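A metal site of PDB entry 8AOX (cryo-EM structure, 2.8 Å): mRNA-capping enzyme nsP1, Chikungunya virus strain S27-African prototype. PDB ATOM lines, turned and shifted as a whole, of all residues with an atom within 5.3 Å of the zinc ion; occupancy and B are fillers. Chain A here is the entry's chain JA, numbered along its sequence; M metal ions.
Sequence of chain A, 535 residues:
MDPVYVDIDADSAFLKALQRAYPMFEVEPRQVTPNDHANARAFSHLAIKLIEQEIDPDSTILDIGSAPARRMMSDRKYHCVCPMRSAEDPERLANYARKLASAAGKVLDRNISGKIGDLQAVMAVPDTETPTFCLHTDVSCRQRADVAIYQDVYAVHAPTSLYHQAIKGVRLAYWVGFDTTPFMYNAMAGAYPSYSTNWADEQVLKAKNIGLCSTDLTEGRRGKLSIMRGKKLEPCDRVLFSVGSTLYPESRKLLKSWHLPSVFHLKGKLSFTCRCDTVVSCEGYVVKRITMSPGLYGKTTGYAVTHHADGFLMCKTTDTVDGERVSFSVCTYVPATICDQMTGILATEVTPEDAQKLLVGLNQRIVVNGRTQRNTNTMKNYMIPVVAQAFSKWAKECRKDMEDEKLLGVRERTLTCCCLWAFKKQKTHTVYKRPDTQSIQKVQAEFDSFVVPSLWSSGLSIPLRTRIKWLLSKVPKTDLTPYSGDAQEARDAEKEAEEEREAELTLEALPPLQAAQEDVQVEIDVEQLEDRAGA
The side-chain carboxylate (OE2) of Glu 129 sits close to the side-chain amide oxygen (OE1) of Gln 143, at 3.2 Å.
The side-chain carboxylate of Glu 129 is in hydrogen-bond range of a ring nitrogen (ND1) of His 136 (3.4 Å).
A ring nitrogen (NE2) of His 79 sits close to the side-chain amide oxygen (OE1) of Gln 143.
SG of Cys 134 lies close to ND1 of His 136 (3.8 Å).
The backbone NH (N) of Gln 143 sits close to the side-chain sulfur (SG) of Cys 141, at 3.3 Å.
Merely in contact with the zinc ion: Gln 143 (3.9 Å).
Along chain A the residues within 4 Å of the zinc ion span positions 79 to 143.
The nearest printed residue that does not touch the zinc ion is Val 81 (4.2 Å).
The zinc ion is bound by OE2 of Glu 129 (2.1 Å), NE2 of His 79 (2.3 Å), SG of Cys 134 (2.3 Å) and SG of Cys 141 (2.3 Å).
The zinc ion has four donor atoms within binding distance.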
ATOM      1  N   HIS A  79     -18.398  -8.721  17.079  1.00  0.00           N
ATOM      2  CA  HIS A  79     -17.315  -9.683  16.881  1.00  0.00           C
ATOM      3  C   HIS A  79     -16.461  -9.682  18.144  1.00  0.00           C
ATOM      4  O   HIS A  79     -15.447  -8.981  18.223  1.00  0.00           O
ATOM      5  CB  HIS A  79     -16.486  -9.348  15.645  1.00  0.00           C
ATOM      6  CG  HIS A  79     -15.960 -10.554  14.927  1.00  0.00           C
ATOM      7  ND1 HIS A  79     -16.691 -11.702  14.746  1.00  0.00           N
ATOM      8  CD2 HIS A  79     -14.741 -10.793  14.391  1.00  0.00           C
ATOM      9  CE1 HIS A  79     -15.959 -12.603  14.113  1.00  0.00           C
ATOM     10  NE2 HIS A  79     -14.757 -12.077  13.896  1.00  0.00           N
ATOM     11  N   VAL A  81     -13.773 -10.569  19.998  1.00  0.00           N
ATOM     12  CA  VAL A  81     -12.467 -11.172  19.756  1.00  0.00           C
ATOM     13  C   VAL A  81     -11.872 -11.626  21.085  1.00  0.00           C
ATOM     14  O   VAL A  81     -11.706 -10.818  22.000  1.00  0.00           O
ATOM     15  CB  VAL A  81     -11.533 -10.190  19.029  1.00  0.00           C
ATOM     16  CG1 VAL A  81     -10.196 -10.838  18.758  1.00  0.00           C
ATOM     17  CG2 VAL A  81     -12.169  -9.713  17.739  1.00  0.00           C
ATOM     18  N   GLU A 129     -13.356 -18.683  11.867  1.00  0.00           N
ATOM     19  CA  GLU A 129     -13.733 -17.275  11.906  1.00  0.00           C
ATOM     20  C   GLU A 129     -15.235 -17.169  11.665  1.00  0.00           C
ATOM     21  O   GLU A 129     -15.699 -16.977  10.544  1.00  0.00           O
ATOM     22  CB  GLU A 129     -12.943 -16.474  10.873  1.00  0.00           C
ATOM     23  CG  GLU A 129     -13.162 -14.972  10.980  1.00  0.00           C
ATOM     24  CD  GLU A 129     -12.531 -14.383  12.211  1.00  0.00           C
ATOM     25  OE1 GLU A 129     -11.520 -14.941  12.694  1.00  0.00           O
ATOM     26  OE2 GLU A 129     -13.046 -13.356  12.711  1.00  0.00           O
ATOM     27  N   CYS A 134     -14.623 -15.327  17.436  1.00  0.00           N
ATOM     28  CA  CYS A 134     -13.394 -15.927  16.930  1.00  0.00           C
ATOM     29  C   CYS A 134     -12.339 -15.894  18.018  1.00  0.00           C
ATOM     30  O   CYS A 134     -12.438 -15.141  18.992  1.00  0.00           O
ATOM     31  CB  CYS A 134     -12.906 -15.217  15.666  1.00  0.00           C
ATOM     32  SG  CYS A 134     -11.754 -13.840  15.933  1.00  0.00           S
ATOM     33  N   HIS A 136      -8.588 -15.255  17.920  1.00  0.00           N
ATOM     34  CA  HIS A 136      -7.356 -14.813  17.286  1.00  0.00           C
ATOM     35  C   HIS A 136      -6.938 -13.490  17.912  1.00  0.00           C
ATOM     36  O   HIS A 136      -7.742 -12.806  18.544  1.00  0.00           O
ATOM     37  CB  HIS A 136      -7.518 -14.643  15.764  1.00  0.00           C
ATOM     38  CG  HIS A 136      -7.834 -15.904  15.041  1.00  0.00           C
ATOM     39  ND1 HIS A 136      -9.128 -16.271  14.717  1.00  0.00           N
ATOM     40  CD2 HIS A 136      -7.035 -16.899  14.577  1.00  0.00           C
ATOM     41  CE1 HIS A 136      -9.109 -17.434  14.086  1.00  0.00           C
ATOM     42  NE2 HIS A 136      -7.852 -17.830  13.989  1.00  0.00           N
ATOM     43  N   CYS A 141      -6.784 -11.803  13.054  1.00  0.00           N
ATOM     44  CA  CYS A 141      -8.166 -12.071  12.686  1.00  0.00           C
ATOM     45  C   CYS A 141      -8.443 -11.565  11.273  1.00  0.00           C
ATOM     46  O   CYS A 141      -7.932 -10.521  10.853  1.00  0.00           O
ATOM     47  CB  CYS A 141      -9.118 -11.414  13.687  1.00  0.00           C
ATOM     48  SG  CYS A 141     -10.831 -11.198  13.109  1.00  0.00           S
ATOM     49  N   ARG A 142      -9.247 -12.316  10.530  1.00  0.00           N
ATOM     50  CA  ARG A 142      -9.515 -12.024   9.132  1.00  0.00           C
ATOM     51  C   ARG A 142     -10.899 -11.423   8.888  1.00  0.00           C
ATOM     52  O   ARG A 142     -11.272 -11.233   7.726  1.00  0.00           O
ATOM     53  CB  ARG A 142      -9.355 -13.291   8.290  1.00  0.00           C
ATOM     54  CG  ARG A 142      -7.959 -13.891   8.331  1.00  0.00           C
ATOM     55  CD  ARG A 142      -7.991 -15.375   7.980  1.00  0.00           C
ATOM     56  NE  ARG A 142      -8.776 -16.142   8.940  1.00  0.00           N
ATOM     57  N   GLN A 143     -11.661 -11.132   9.939  1.00  0.00           N
ATOM     58  CA  GLN A 143     -12.968 -10.526   9.758  1.00  0.00           C
ATOM     59  C   GLN A 143     -12.829  -9.111   9.211  1.00  0.00           C
ATOM     60  O   GLN A 143     -11.900  -8.377   9.556  1.00  0.00           O
ATOM     61  CB  GLN A 143     -13.743 -10.511  11.074  1.00  0.00           C
ATOM     62  CG  GLN A 143     -15.206 -10.122  10.944  1.00  0.00           C
ATOM     63  CD  GLN A 143     -16.113 -11.334  10.822  1.00  0.00           C
ATOM     64  OE1 GLN A 143     -15.714 -12.461  11.118  1.00  0.00           O
ATOM     65  NE2 GLN A 143     -17.350 -11.111  10.407  1.00  0.00           N
HETATM   66 ZN    ZN M   1     -12.486 -12.264  14.377  1.00  0.00          ZN
